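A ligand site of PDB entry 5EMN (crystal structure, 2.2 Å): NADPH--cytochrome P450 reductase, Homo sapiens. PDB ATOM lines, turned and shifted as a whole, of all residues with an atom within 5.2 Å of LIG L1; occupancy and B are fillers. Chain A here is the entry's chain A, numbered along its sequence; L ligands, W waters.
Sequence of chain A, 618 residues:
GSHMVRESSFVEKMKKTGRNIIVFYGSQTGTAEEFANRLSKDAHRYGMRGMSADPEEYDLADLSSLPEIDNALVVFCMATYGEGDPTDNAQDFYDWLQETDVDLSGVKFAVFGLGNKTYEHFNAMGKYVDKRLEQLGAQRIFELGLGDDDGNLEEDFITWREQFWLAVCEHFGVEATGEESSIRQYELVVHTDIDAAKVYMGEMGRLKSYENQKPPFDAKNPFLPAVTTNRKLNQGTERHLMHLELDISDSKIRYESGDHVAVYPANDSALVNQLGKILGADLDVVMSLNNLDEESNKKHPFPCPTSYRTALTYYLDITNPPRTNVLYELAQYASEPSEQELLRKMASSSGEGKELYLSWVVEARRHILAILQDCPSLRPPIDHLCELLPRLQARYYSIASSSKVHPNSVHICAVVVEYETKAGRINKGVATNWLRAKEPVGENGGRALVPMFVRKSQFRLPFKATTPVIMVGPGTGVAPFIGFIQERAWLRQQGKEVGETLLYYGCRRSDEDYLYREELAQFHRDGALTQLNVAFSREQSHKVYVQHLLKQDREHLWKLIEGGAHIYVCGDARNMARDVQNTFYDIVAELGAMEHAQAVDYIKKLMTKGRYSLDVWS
Residues that only touch LIG L1: Gly 115, Ala 79, Tyr 119, Gly 30, Phe 122, Leu 153, Gly 84, Asp 149 and Gly 82.
Hydrophobic or aromatic side chains within 4 Å of LIG L1: Ala 32, Ala 79, Tyr 81, Leu 114, Tyr 119, Phe 122 and Leu 153.
Within 4 Å of LIG L1: Ser 27, Gln 28, Thr 29, Gly 30, Thr 31, Ala 32, Ala 79, Thr 80, Tyr 81, Gly 82, Gly 84, Leu 114, Gly 115, Asn 116, Tyr 119, His 121, Phe 122, Asn 123, Asp 149 and Leu 153.
Along chain A the residues within 4 Å of LIG L1 span positions 27 to 153.
An oxygen (O8) of LIG L1 sits at hydrogen-bond distance from the backbone NH of Thr 29, 3.0 Å away.
An oxygen (O7) of LIG L1 sits at hydrogen-bond distance from the side-chain hydroxyl of Thr 29.
N of Thr 31 sits at hydrogen-bond distance from O7 of LIG L1, 3.0 Å away.
The side-chain hydroxyl of Thr 31 sits at hydrogen-bond distance from an oxygen (O7) of LIG L1 (2.5 Å).
O9 of LIG L1 sits at hydrogen-bond distance from OG of Ser 27 (2.5 Å).
The backbone NH (N) of Ala 32 sits at hydrogen-bond distance from an oxygen (O9) of LIG L1 (2.6 Å).
O3 of LIG L1 lies within hydrogen-bond range of N of Thr 80.
An oxygen (O3) of LIG L1 lies within hydrogen-bond range of the backbone carbonyl oxygen (O) of Thr 80.
An oxygen (O8) of LIG L1 sits at hydrogen-bond distance from the side-chain hydroxyl (OH) of Tyr 81 (2.7 Å).
The backbone NH (N) of Gln 28 sits at hydrogen-bond distance from an oxygen (O8) of LIG L1 (2.8 Å).
An oxygen (O1) of LIG L1 is in hydrogen-bond range of the backbone NH (N) of Asn 116 (2.9 Å).
An oxygen (O1) of LIG L1 lies within hydrogen-bond range of the backbone NH of Asn 123, 2.9 Å away.
N2 of LIG L1 sits at hydrogen-bond distance from O of His 121 (3.1 Å).
An oxygen (O3) of LIG L1 sits at hydrogen-bond distance from the backbone carbonyl oxygen of Leu 114, 3.3 Å away.
O of Tyr 396 lies within hydrogen-bond range of O9 of LG2 L2, at 2.8 Å.
Water W2 lies within hydrogen-bond range of an oxygen (O5) of LIG L1 (2.8 Å) and the side-chain hydroxyl (OG1) of Thr 31 (2.8 Å).
Water W1 bridges N of His 121 (2.7 Å) and O2 of LIG L1 (2.8 Å).
The side-chain hydroxyl (OG) of Ser 27 sits at hydrogen-bond distance from the backbone NH (N) of Gly 30.
The backbone NH (N) of Ser 27 lies within hydrogen-bond range of the side-chain hydroxyl (OG1) of Thr 87 (3.5 Å).
The side-chain hydroxyl of Thr 80 sits at hydrogen-bond distance from the backbone NH of Ala 124 (3.3 Å).
NE2 of Gln 28 lies within hydrogen-bond range of OH of Tyr 396, 3.0 Å away.
The side-chain amide oxygen of Asn 123 is in hydrogen-bond range of the backbone NH of Gly 115 (3.1 Å).
OD1 of Asn 123 sits close to O of Leu 114 (3.2 Å).
The backbone carbonyl oxygen (O) of Gly 115 sits at hydrogen-bond distance from the backbone NH (N) of Asp 149 (2.8 Å).
The backbone carbonyl oxygen (O) of Gly 26 is in hydrogen-bond range of the backbone NH (N) of Ala 79, 3.0 Å away.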
ATOM      1  N   GLY A  26     -24.987  11.298   2.056  1.00  0.00           N
ATOM      2  CA  GLY A  26     -25.785  10.208   1.538  1.00  0.00           C
ATOM      3  C   GLY A  26     -25.244   9.046   2.335  1.00  0.00           C
ATOM      4  O   GLY A  26     -24.142   8.583   2.041  1.00  0.00           O
ATOM      5  N   SER A  27     -25.994   8.567   3.319  1.00  0.00           N
ATOM      6  CA  SER A  27     -25.490   7.517   4.196  1.00  0.00           C
ATOM      7  C   SER A  27     -26.526   6.473   4.586  1.00  0.00           C
ATOM      8  O   SER A  27     -27.693   6.790   4.786  1.00  0.00           O
ATOM      9  CB  SER A  27     -24.948   8.181   5.468  1.00  0.00           C
ATOM     10  OG  SER A  27     -24.358   7.239   6.340  1.00  0.00           O
ATOM     11  N   GLN A  28     -26.082   5.226   4.708  1.00  0.00           N
ATOM     12  CA  GLN A  28     -26.993   4.163   5.114  1.00  0.00           C
ATOM     13  C   GLN A  28     -26.594   3.664   6.509  1.00  0.00           C
ATOM     14  O   GLN A  28     -27.462   3.359   7.333  1.00  0.00           O
ATOM     15  CB  GLN A  28     -26.994   2.990   4.122  1.00  0.00           C
ATOM     16  CG  GLN A  28     -28.035   1.925   4.471  1.00  0.00           C
ATOM     17  CD  GLN A  28     -28.086   0.769   3.469  1.00  0.00           C
ATOM     18  OE1 GLN A  28     -28.406   0.968   2.293  1.00  0.00           O
ATOM     19  NE2 GLN A  28     -27.788  -0.441   3.940  1.00  0.00           N
ATOM     20  N   THR A  29     -25.285   3.604   6.784  1.00  0.00           N
ATOM     21  CA  THR A  29     -24.806   3.165   8.100  1.00  0.00           C
ATOM     22  C   THR A  29     -24.020   4.202   8.911  1.00  0.00           C
ATOM     23  O   THR A  29     -23.150   3.860   9.703  1.00  0.00           O
ATOM     24  CB  THR A  29     -23.981   1.836   8.010  1.00  0.00           C
ATOM     25  OG1 THR A  29     -22.841   2.016   7.167  1.00  0.00           O
ATOM     26  CG2 THR A  29     -24.851   0.714   7.445  1.00  0.00           C
ATOM     27  N   GLY A  30     -24.351   5.472   8.688  1.00  0.00           N
ATOM     28  CA  GLY A  30     -23.747   6.565   9.434  1.00  0.00           C
ATOM     29  C   GLY A  30     -22.393   7.159   9.094  1.00  0.00           C
ATOM     30  O   GLY A  30     -22.133   8.305   9.446  1.00  0.00           O
ATOM     31  N   THR A  31     -21.532   6.410   8.411  1.00  0.00           N
ATOM     32  CA  THR A  31     -20.192   6.903   8.103  1.00  0.00           C
ATOM     33  C   THR A  31     -20.130   8.219   7.317  1.00  0.00           C
ATOM     34  O   THR A  31     -19.392   9.122   7.681  1.00  0.00           O
ATOM     35  CB  THR A  31     -19.371   5.870   7.292  1.00  0.00           C
ATOM     36  OG1 THR A  31     -19.784   4.542   7.610  1.00  0.00           O
ATOM     37  CG2 THR A  31     -17.887   6.021   7.636  1.00  0.00           C
ATOM     38  N   ALA A  32     -20.880   8.321   6.227  1.00  0.00           N
ATOM     39  CA  ALA A  32     -20.851   9.538   5.433  1.00  0.00           C
ATOM     40  C   ALA A  32     -21.428  10.657   6.301  1.00  0.00           C
ATOM     41  O   ALA A  32     -20.955  11.801   6.258  1.00  0.00           O
ATOM     42  CB  ALA A  32     -21.698   9.369   4.149  1.00  0.00           C
ATOM     43  N   GLU A  33     -22.418  10.312   7.107  1.00  0.00           N
ATOM     44  CA  GLU A  33     -23.065  11.283   7.982  1.00  0.00           C
ATOM     45  C   GLU A  33     -22.049  11.839   8.990  1.00  0.00           C
ATOM     46  O   GLU A  33     -22.027  13.047   9.248  1.00  0.00           O
ATOM     47  CB  GLU A  33     -24.243  10.635   8.715  1.00  0.00           C
ATOM     48  CG  GLU A  33     -24.946  11.586   9.684  1.00  0.00           C
ATOM     49  CD  GLU A  33     -26.247  11.014  10.202  1.00  0.00           C
ATOM     50  OE1 GLU A  33     -27.050  11.807  10.754  1.00  0.00           O
ATOM     51  OE2 GLU A  33     -26.475   9.783  10.062  1.00  0.00           O
ATOM     52  N   ALA A  79     -22.098   7.897  -0.036  1.00  0.00           N
ATOM     53  CA  ALA A  79     -21.744   6.494  -0.054  1.00  0.00           C
ATOM     54  C   ALA A  79     -22.445   5.854  -1.246  1.00  0.00           C
ATOM     55  O   ALA A  79     -23.490   6.333  -1.681  1.00  0.00           O
ATOM     56  CB  ALA A  79     -22.201   5.816   1.238  1.00  0.00           C
ATOM     57  N   THR A  80     -21.855   4.784  -1.777  1.00  0.00           N
ATOM     58  CA  THR A  80     -22.430   4.043  -2.902  1.00  0.00           C
ATOM     59  C   THR A  80     -22.893   2.677  -2.383  1.00  0.00           C
ATOM     60  O   THR A  80     -22.229   2.071  -1.550  1.00  0.00           O
ATOM     61  CB  THR A  80     -21.409   3.799  -4.022  1.00  0.00           C
ATOM     62  OG1 THR A  80     -20.972   5.055  -4.550  1.00  0.00           O
ATOM     63  CG2 THR A  80     -22.043   2.985  -5.134  1.00  0.00           C
ATOM     64  N   TYR A  81     -24.049   2.232  -2.864  1.00  0.00           N
ATOM     65  CA  TYR A  81     -24.620   0.945  -2.468  1.00  0.00           C
ATOM     66  C   TYR A  81     -24.878  -0.011  -3.623  1.00  0.00           C
ATOM     67  O   TYR A  81     -24.194   0.041  -4.653  1.00  0.00           O
ATOM     68  CB  TYR A  81     -25.754   1.145  -1.460  1.00  0.00           C
ATOM     69  CG  TYR A  81     -25.269   1.256  -0.038  1.00  0.00           C
ATOM     70  CD1 TYR A  81     -24.652   2.420   0.415  1.00  0.00           C
ATOM     71  CD2 TYR A  81     -25.386   0.177   0.845  1.00  0.00           C
ATOM     72  CE1 TYR A  81     -24.164   2.513   1.710  1.00  0.00           C
ATOM     73  CE2 TYR A  81     -24.893   0.264   2.147  1.00  0.00           C
ATOM     74  CZ  TYR A  81     -24.279   1.443   2.571  1.00  0.00           C
ATOM     75  OH  TYR A  81     -23.746   1.531   3.833  1.00  0.00           O
ATOM     76  N   GLY A  82     -25.881  -0.868  -3.454  1.00  0.00           N
ATOM     77  CA  GLY A  82     -26.245  -1.816  -4.491  1.00  0.00           C
ATOM     78  C   GLY A  82     -26.043  -1.395  -5.931  1.00  0.00           C
ATOM     79  O   GLY A  82     -26.748  -0.506  -6.414  1.00  0.00           O
ATOM     80  N   GLU A  83     -25.341  -2.166  -6.709  1.00  0.00           N
ATOM     81  CA  GLU A  83     -25.096  -1.877  -8.120  1.00  0.00           C
ATOM     82  C   GLU A  83     -24.656  -0.474  -8.556  1.00  0.00           C
ATOM     83  O   GLU A  83     -25.036   0.009  -9.622  1.00  0.00           O
ATOM     84  CB  GLU A  83     -26.453  -2.102  -8.785  1.00  0.00           C
ATOM     85  CG  GLU A  83     -26.785  -3.557  -9.050  1.00  0.00           C
ATOM     86  CD  GLU A  83     -28.185  -3.926  -8.612  1.00  0.00           C
ATOM     87  OE1 GLU A  83     -28.482  -3.820  -7.395  1.00  0.00           O
ATOM     88  OE2 GLU A  83     -29.006  -4.316  -9.470  1.00  0.00           O
ATOM     89  N   GLY A  84     -23.874   0.196  -7.704  1.00  0.00           N
ATOM     90  CA  GLY A  84     -23.523   1.579  -7.884  1.00  0.00           C
ATOM     91  C   GLY A  84     -24.689   2.531  -7.778  1.00  0.00           C
ATOM     92  O   GLY A  84     -24.804   3.475  -8.553  1.00  0.00           O
ATOM     93  N   THR A  87     -27.720   5.869  -1.742  1.00  0.00           N
ATOM     94  CA  THR A  87     -28.342   5.446  -0.505  1.00  0.00           C
ATOM     95  C   THR A  87     -29.802   5.902  -0.629  1.00  0.00           C
ATOM     96  O   THR A  87     -30.122   6.786  -1.425  1.00  0.00           O
ATOM     97  CB  THR A  87     -27.701   6.139   0.681  1.00  0.00           C
ATOM     98  OG1 THR A  87     -27.660   7.553   0.432  1.00  0.00           O
ATOM     99  CG2 THR A  87     -26.275   5.630   0.899  1.00  0.00           C
ATOM    100  N   LEU A 114     -17.692   7.828  -0.653  1.00  0.00           N
ATOM    101  CA  LEU A 114     -17.351   6.687   0.193  1.00  0.00           C
ATOM    102  C   LEU A 114     -17.693   5.444  -0.584  1.00  0.00           C
ATOM    103  O   LEU A 114     -18.847   5.275  -0.976  1.00  0.00           O
ATOM    104  CB  LEU A 114     -18.153   6.663   1.491  1.00  0.00           C
ATOM    105  CG  LEU A 114     -17.886   7.725   2.549  1.00  0.00           C
ATOM    106  CD1 LEU A 114     -18.388   9.080   2.080  1.00  0.00           C
ATOM    107  CD2 LEU A 114     -18.582   7.279   3.832  1.00  0.00           C
ATOM    108  N   GLY A 115     -16.696   4.591  -0.801  1.00  0.00           N
ATOM    109  CA  GLY A 115     -16.915   3.354  -1.542  1.00  0.00           C
ATOM    110  C   GLY A 115     -16.024   2.214  -1.086  1.00  0.00           C
ATOM    111  O   GLY A 115     -15.397   2.276  -0.018  1.00  0.00           O
ATOM    112  N   ASN A 116     -15.988   1.163  -1.886  1.00  0.00           N
ATOM    113  CA  ASN A 116     -15.173  -0.014  -1.589  1.00  0.00           C
ATOM    114  C   ASN A 116     -14.792  -0.576  -2.944  1.00  0.00           C
ATOM    115  O   ASN A 116     -15.650  -0.896  -3.741  1.00  0.00           O
ATOM    116  CB  ASN A 116     -16.011  -1.039  -0.823  1.00  0.00           C
ATOM    117  CG  ASN A 116     -15.198  -2.213  -0.312  1.00  0.00           C
ATOM    118  OD1 ASN A 116     -14.368  -2.779  -1.038  1.00  0.00           O
ATOM    119  ND2 ASN A 116     -15.422  -2.592   0.947  1.00  0.00           N
ATOM    120  N   LYS A 117     -13.500  -0.700  -3.226  1.00  0.00           N
ATOM    121  CA  LYS A 117     -13.091  -1.200  -4.525  1.00  0.00           C
ATOM    122  C   LYS A 117     -13.304  -2.704  -4.778  1.00  0.00           C
ATOM    123  O   LYS A 117     -12.980  -3.196  -5.847  1.00  0.00           O
ATOM    124  CB  LYS A 117     -11.648  -0.784  -4.816  1.00  0.00           C
ATOM    125  CG  LYS A 117     -10.604  -1.287  -3.835  1.00  0.00           C
ATOM    126  CD  LYS A 117      -9.218  -0.748  -4.195  1.00  0.00           C
ATOM    127  CE  LYS A 117      -8.097  -1.528  -3.483  1.00  0.00           C
ATOM    128  NZ  LYS A 117      -8.147  -1.448  -1.985  1.00  0.00           N
ATOM    129  N   TYR A 119     -16.174  -3.929  -4.847  1.00  0.00           N
ATOM    130  CA  TYR A 119     -17.499  -3.936  -5.471  1.00  0.00           C
ATOM    131  C   TYR A 119     -17.352  -3.569  -6.943  1.00  0.00           C
ATOM    132  O   TYR A 119     -16.361  -2.954  -7.338  1.00  0.00           O
ATOM    133  CB  TYR A 119     -18.432  -2.946  -4.773  1.00  0.00           C
ATOM    134  CG  TYR A 119     -18.903  -3.420  -3.420  1.00  0.00           C
ATOM    135  CD1 TYR A 119     -19.956  -4.328  -3.313  1.00  0.00           C
ATOM    136  CD2 TYR A 119     -18.265  -3.001  -2.251  1.00  0.00           C
ATOM    137  CE1 TYR A 119     -20.358  -4.809  -2.067  1.00  0.00           C
ATOM    138  CE2 TYR A 119     -18.664  -3.488  -1.012  1.00  0.00           C
ATOM    139  CZ  TYR A 119     -19.701  -4.386  -0.921  1.00  0.00           C
ATOM    140  OH  TYR A 119     -20.085  -4.881   0.303  1.00  0.00           O
ATOM    141  N   HIS A 121     -19.102  -1.407  -8.977  1.00  0.00           N
ATOM    142  CA  HIS A 121     -19.130   0.010  -9.333  1.00  0.00           C
ATOM    143  C   HIS A 121     -18.520   0.859  -8.222  1.00  0.00           C
ATOM    144  O   HIS A 121     -19.226   1.366  -7.354  1.00  0.00           O
ATOM    145  CB  HIS A 121     -20.556   0.442  -9.637  1.00  0.00           C
ATOM    146  CG  HIS A 121     -21.210  -0.368 -10.704  1.00  0.00           C
ATOM    147  ND1 HIS A 121     -21.898  -1.532 -10.449  1.00  0.00           N
ATOM    148  CD2 HIS A 121     -21.269  -0.186 -12.050  1.00  0.00           C
ATOM    149  CE1 HIS A 121     -22.358  -2.028 -11.582  1.00  0.00           C
ATOM    150  NE2 HIS A 121     -21.992  -1.243 -12.566  1.00  0.00           N
ATOM    151  N   PHE A 122     -17.200   0.978  -8.257  1.00  0.00           N
ATOM    152  CA  PHE A 122     -16.485   1.717  -7.240  1.00  0.00           C
ATOM    153  C   PHE A 122     -16.803   3.204  -7.184  1.00  0.00           C
ATOM    154  O   PHE A 122     -16.511   3.949  -8.121  1.00  0.00           O
ATOM    155  CB  PHE A 122     -14.989   1.535  -7.403  1.00  0.00           C
ATOM    156  CG  PHE A 122     -14.159   2.299  -6.401  1.00  0.00           C
ATOM    157  CD1 PHE A 122     -14.401   2.139  -5.038  1.00  0.00           C
ATOM    158  CD2 PHE A 122     -13.146   3.149  -6.820  1.00  0.00           C
ATOM    159  CE1 PHE A 122     -13.626   2.840  -4.102  1.00  0.00           C
ATOM    160  CE2 PHE A 122     -12.367   3.861  -5.893  1.00  0.00           C
ATOM    161  CZ  PHE A 122     -12.609   3.701  -4.530  1.00  0.00           C
ATOM    162  N   ASN A 123     -17.403   3.617  -6.063  1.00  0.00           N
ATOM    163  CA  ASN A 123     -17.743   4.999  -5.831  1.00  0.00           C
ATOM    164  C   ASN A 123     -18.600   5.589  -6.941  1.00  0.00           C
ATOM    165  O   ASN A 123     -18.490   6.768  -7.269  1.00  0.00           O
ATOM    166  CB  ASN A 123     -16.468   5.830  -5.649  1.00  0.00           C
ATOM    167  CG  ASN A 123     -16.134   6.088  -4.188  1.00  0.00           C
ATOM    168  OD1 ASN A 123     -17.033   6.271  -3.362  1.00  0.00           O
ATOM    169  ND2 ASN A 123     -14.842   6.068  -3.857  1.00  0.00           N
ATOM    170  N   ALA A 124     -19.472   4.763  -7.511  1.00  0.00           N
ATOM    171  CA  ALA A 124     -20.340   5.229  -8.594  1.00  0.00           C
ATOM    172  C   ALA A 124     -21.108   6.466  -8.173  1.00  0.00           C
ATOM    173  O   ALA A 124     -21.213   7.418  -8.934  1.00  0.00           O
ATOM    174  CB  ALA A 124     -21.309   4.128  -9.021  1.00  0.00           C
ATOM    175  N   ASP A 149     -13.068   1.948   1.512  1.00  0.00           N
ATOM    176  CA  ASP A 149     -13.228   1.186   2.729  1.00  0.00           C
ATOM    177  C   ASP A 149     -12.591  -0.217   2.666  1.00  0.00           C
ATOM    178  O   ASP A 149     -12.761  -1.026   3.574  1.00  0.00           O
ATOM    179  CB  ASP A 149     -14.717   1.096   3.080  1.00  0.00           C
ATOM    180  CG  ASP A 149     -14.960   0.546   4.494  1.00  0.00           C
ATOM    181  OD1 ASP A 149     -14.341   1.051   5.458  1.00  0.00           O
ATOM    182  OD2 ASP A 149     -15.781  -0.395   4.621  1.00  0.00           O
ATOM    183  N   LEU A 153     -10.672   3.895   4.833  1.00  0.00           N
ATOM    184  CA  LEU A 153     -11.482   5.048   4.473  1.00  0.00           C
ATOM    185  C   LEU A 153     -11.083   6.262   5.332  1.00  0.00           C
ATOM    186  O   LEU A 153     -10.897   7.369   4.816  1.00  0.00           O
ATOM    187  CB  LEU A 153     -12.972   4.718   4.676  1.00  0.00           C
ATOM    188  CG  LEU A 153     -13.999   5.760   4.250  1.00  0.00           C
ATOM    189  CD1 LEU A 153     -13.873   6.002   2.742  1.00  0.00           C
ATOM    190  CD2 LEU A 153     -15.395   5.291   4.612  1.00  0.00           C
ATOM    191  N   TYR A 396     -26.520  -6.796   8.485  1.00  0.00           N
ATOM    192  CA  TYR A 396     -27.337  -7.408   7.432  1.00  0.00           C
ATOM    193  C   TYR A 396     -26.964  -8.870   7.232  1.00  0.00           C
ATOM    194  O   TYR A 396     -25.783  -9.248   7.301  1.00  0.00           O
ATOM    195  CB  TYR A 396     -27.147  -6.645   6.112  1.00  0.00           C
ATOM    196  CG  TYR A 396     -27.492  -5.166   6.193  1.00  0.00           C
ATOM    197  CD1 TYR A 396     -28.830  -4.737   6.251  1.00  0.00           C
ATOM    198  CD2 TYR A 396     -26.486  -4.201   6.314  1.00  0.00           C
ATOM    199  CE1 TYR A 396     -29.149  -3.384   6.419  1.00  0.00           C
ATOM    200  CE2 TYR A 396     -26.797  -2.842   6.480  1.00  0.00           C
ATOM    201  CZ  TYR A 396     -28.136  -2.448   6.542  1.00  0.00           C
ATOM    202  OH  TYR A 396     -28.446  -1.121   6.797  1.00  0.00           O
HETATM  203  N1  LIG L   1     -19.034   0.629  -2.300  1.00  0.00           N
HETATM  204  C1  LIG L   1     -18.844   0.917  -3.605  1.00  0.00           C
HETATM  205  O1  LIG L   1     -17.882   1.599  -3.988  1.00  0.00           O
HETATM  206  N2  LIG L   1     -19.767   0.399  -4.491  1.00  0.00           N
HETATM  207  C2  LIG L   1     -20.881  -0.385  -4.195  1.00  0.00           C
HETATM  208  O2  LIG L   1     -21.543  -0.714  -5.156  1.00  0.00           O
HETATM  209  C3  LIG L   1     -21.088  -0.709  -2.835  1.00  0.00           C
HETATM  210  N3  LIG L   1     -22.201  -1.542  -2.507  1.00  0.00           N
HETATM  211  C4  LIG L   1     -22.307  -1.816  -1.148  1.00  0.00           C
HETATM  212  C5  LIG L   1     -23.414  -2.661  -0.762  1.00  0.00           C
HETATM  213  C6  LIG L   1     -23.635  -3.020   0.596  1.00  0.00           C
HETATM  214  C7  LIG L   1     -24.845  -3.935   0.885  1.00  0.00           C
HETATM  215  C8  LIG L   1     -22.725  -2.524   1.671  1.00  0.00           C
HETATM  216  C9  LIG L   1     -22.820  -2.799   3.021  1.00  0.00           C
HETATM  217  C10 LIG L   1     -21.666  -1.710   1.307  1.00  0.00           C
HETATM  218  C11 LIG L   1     -21.418  -1.326  -0.077  1.00  0.00           C
HETATM  219  N4  LIG L   1     -20.313  -0.474  -0.514  1.00  0.00           N
HETATM  220  C12 LIG L   1     -20.120  -0.160  -1.928  1.00  0.00           C
HETATM  221  C13 LIG L   1     -19.398   0.067   0.478  1.00  0.00           C
HETATM  222  C14 LIG L   1     -19.933   1.395   1.123  1.00  0.00           C
HETATM  223  O3  LIG L   1     -20.140   2.400   0.046  1.00  0.00           O
HETATM  224  C15 LIG L   1     -18.938   1.895   2.145  1.00  0.00           C
HETATM  225  O4  LIG L   1     -18.848   0.846   3.153  1.00  0.00           O
HETATM  226  C16 LIG L   1     -19.460   3.249   2.757  1.00  0.00           C
HETATM  227  O5  LIG L   1     -18.373   3.597   3.662  1.00  0.00           O
HETATM  228  C17 LIG L   1     -20.671   3.134   3.652  1.00  0.00           C
HETATM  229  O6  LIG L   1     -21.108   4.456   4.143  1.00  0.00           O
HETATM  230  P1  LIG L   1     -22.307   4.716   5.138  1.00  0.00           P
HETATM  231  O7  LIG L   1     -21.944   4.183   6.475  1.00  0.00           O
HETATM  232  O8  LIG L   1     -23.562   4.150   4.393  1.00  0.00           O
HETATM  233  O9  LIG L   1     -22.273   6.318   5.215  1.00  0.00           O
HETATM  234  P1  LG2 L   2     -18.287  -7.020  14.138  1.00  0.00           P
HETATM  235  O1  LG2 L   2     -18.231  -6.675  15.579  1.00  0.00           O
HETATM  236  O2  LG2 L   2     -18.991  -6.103  13.210  1.00  0.00           O
HETATM  237  O3  LG2 L   2     -16.783  -7.237  13.606  1.00  0.00           O
HETATM  238  C1  LG2 L   2     -16.523  -7.371  12.211  1.00  0.00           C
HETATM  239  C2  LG2 L   2     -15.061  -6.975  11.948  1.00  0.00           C
HETATM  240  O4  LG2 L   2     -14.171  -7.796  12.711  1.00  0.00           O
HETATM  241  C3  LG2 L   2     -14.655  -7.301  10.526  1.00  0.00           C
HETATM  242  O5  LG2 L   2     -15.184  -6.285   9.655  1.00  0.00           O
HETATM  243  C4  LG2 L   2     -13.163  -7.098  10.692  1.00  0.00           C
HETATM  244  O6  LG2 L   2     -12.856  -5.690  10.700  1.00  0.00           O
HETATM  245  C5  LG2 L   2     -12.895  -7.701  12.054  1.00  0.00           C
HETATM  246  N1  LG2 L   2     -12.355  -9.075  11.964  1.00  0.00           N
HETATM  247  C6  LG2 L   2     -13.141 -10.312  11.793  1.00  0.00           C
HETATM  248  N2  LG2 L   2     -12.070 -11.324  11.818  1.00  0.00           N
HETATM  249  C7  LG2 L   2     -10.902 -10.708  11.967  1.00  0.00           C
HETATM  250  C8  LG2 L   2      -9.671 -11.232  12.051  1.00  0.00           C
HETATM  251  N3  LG2 L   2      -9.603 -12.551  12.100  1.00  0.00           N
HETATM  252  N4  LG2 L   2      -8.573 -10.468  12.145  1.00  0.00           N
HETATM  253  C9  LG2 L   2      -8.708  -9.081  12.175  1.00  0.00           C
HETATM  254  N5  LG2 L   2     -10.002  -8.558  12.077  1.00  0.00           N
HETATM  255  C10 LG2 L   2     -11.058  -9.386  11.977  1.00  0.00           C
HETATM  256  N6  LG2 L   2     -22.525 -12.609   7.442  1.00  0.00           N
HETATM  257  C11 LG2 L   2     -22.980 -13.916   7.663  1.00  0.00           C
HETATM  258  O7  LG2 L   2     -22.365 -14.648   8.434  1.00  0.00           O
HETATM  259  N7  LG2 L   2     -24.089 -14.402   6.952  1.00  0.00           N
HETATM  260  C12 LG2 L   2     -24.731 -13.581   6.011  1.00  0.00           C
HETATM  261  O8  LG2 L   2     -25.718 -13.999   5.423  1.00  0.00           O
HETATM  262  C13 LG2 L   2     -24.254 -12.293   5.776  1.00  0.00           C
HETATM  263  N8  LG2 L   2     -24.758 -11.569   4.772  1.00  0.00           N
HETATM  264  C14 LG2 L   2     -24.308 -10.324   4.565  1.00  0.00           C
HETATM  265  C15 LG2 L   2     -24.870  -9.553   3.548  1.00  0.00           C
HETATM  266  C16 LG2 L   2     -24.460  -8.241   3.361  1.00  0.00           C
HETATM  267  C17 LG2 L   2     -25.114  -7.436   2.431  1.00  0.00           C
HETATM  268  C18 LG2 L   2     -23.466  -7.703   4.173  1.00  0.00           C
HETATM  269  C19 LG2 L   2     -23.035  -6.385   3.990  1.00  0.00           C
HETATM  270  C20 LG2 L   2     -22.904  -8.474   5.189  1.00  0.00           C
HETATM  271  C21 LG2 L   2     -23.337  -9.783   5.393  1.00  0.00           C
HETATM  272  N9  LG2 L   2     -22.840 -10.513   6.398  1.00  0.00           N
HETATM  273  C22 LG2 L   2     -23.166 -11.813   6.483  1.00  0.00           C
HETATM  274  C23 LG2 L   2     -21.824  -9.975   7.337  1.00  0.00           C
HETATM  275  C24 LG2 L   2     -22.526  -9.432   8.579  1.00  0.00           C
HETATM  276  O9  LG2 L   2     -23.312  -8.297   8.218  1.00  0.00           O
HETATM  277  C25 LG2 L   2     -21.550  -9.028   9.684  1.00  0.00           C
HETATM  278  O10 LG2 L   2     -20.536  -8.171   9.157  1.00  0.00           O
HETATM  279  C26 LG2 L   2     -20.897 -10.254  10.332  1.00  0.00           C
HETATM  280  O11 LG2 L   2     -21.894 -11.152  10.803  1.00  0.00           O
HETATM  281  C27 LG2 L   2     -20.019  -9.795  11.499  1.00  0.00           C
HETATM  282  O12 LG2 L   2     -20.775  -8.939  12.362  1.00  0.00           O
HETATM  283  P2  LG2 L   2     -20.466  -8.832  13.939  1.00  0.00           P
HETATM  284  O13 LG2 L   2     -20.665 -10.166  14.563  1.00  0.00           O
HETATM  285  O14 LG2 L   2     -21.225  -7.687  14.482  1.00  0.00           O
HETATM  286  O15 LG2 L   2     -18.894  -8.511  13.971  1.00  0.00           O
HETATM  287  O   HOH W   1     -21.080  -2.324  -7.381  1.00  0.00           O
HETATM  288  O   HOH W   2     -18.226   2.597   6.245  1.00  0.00           O
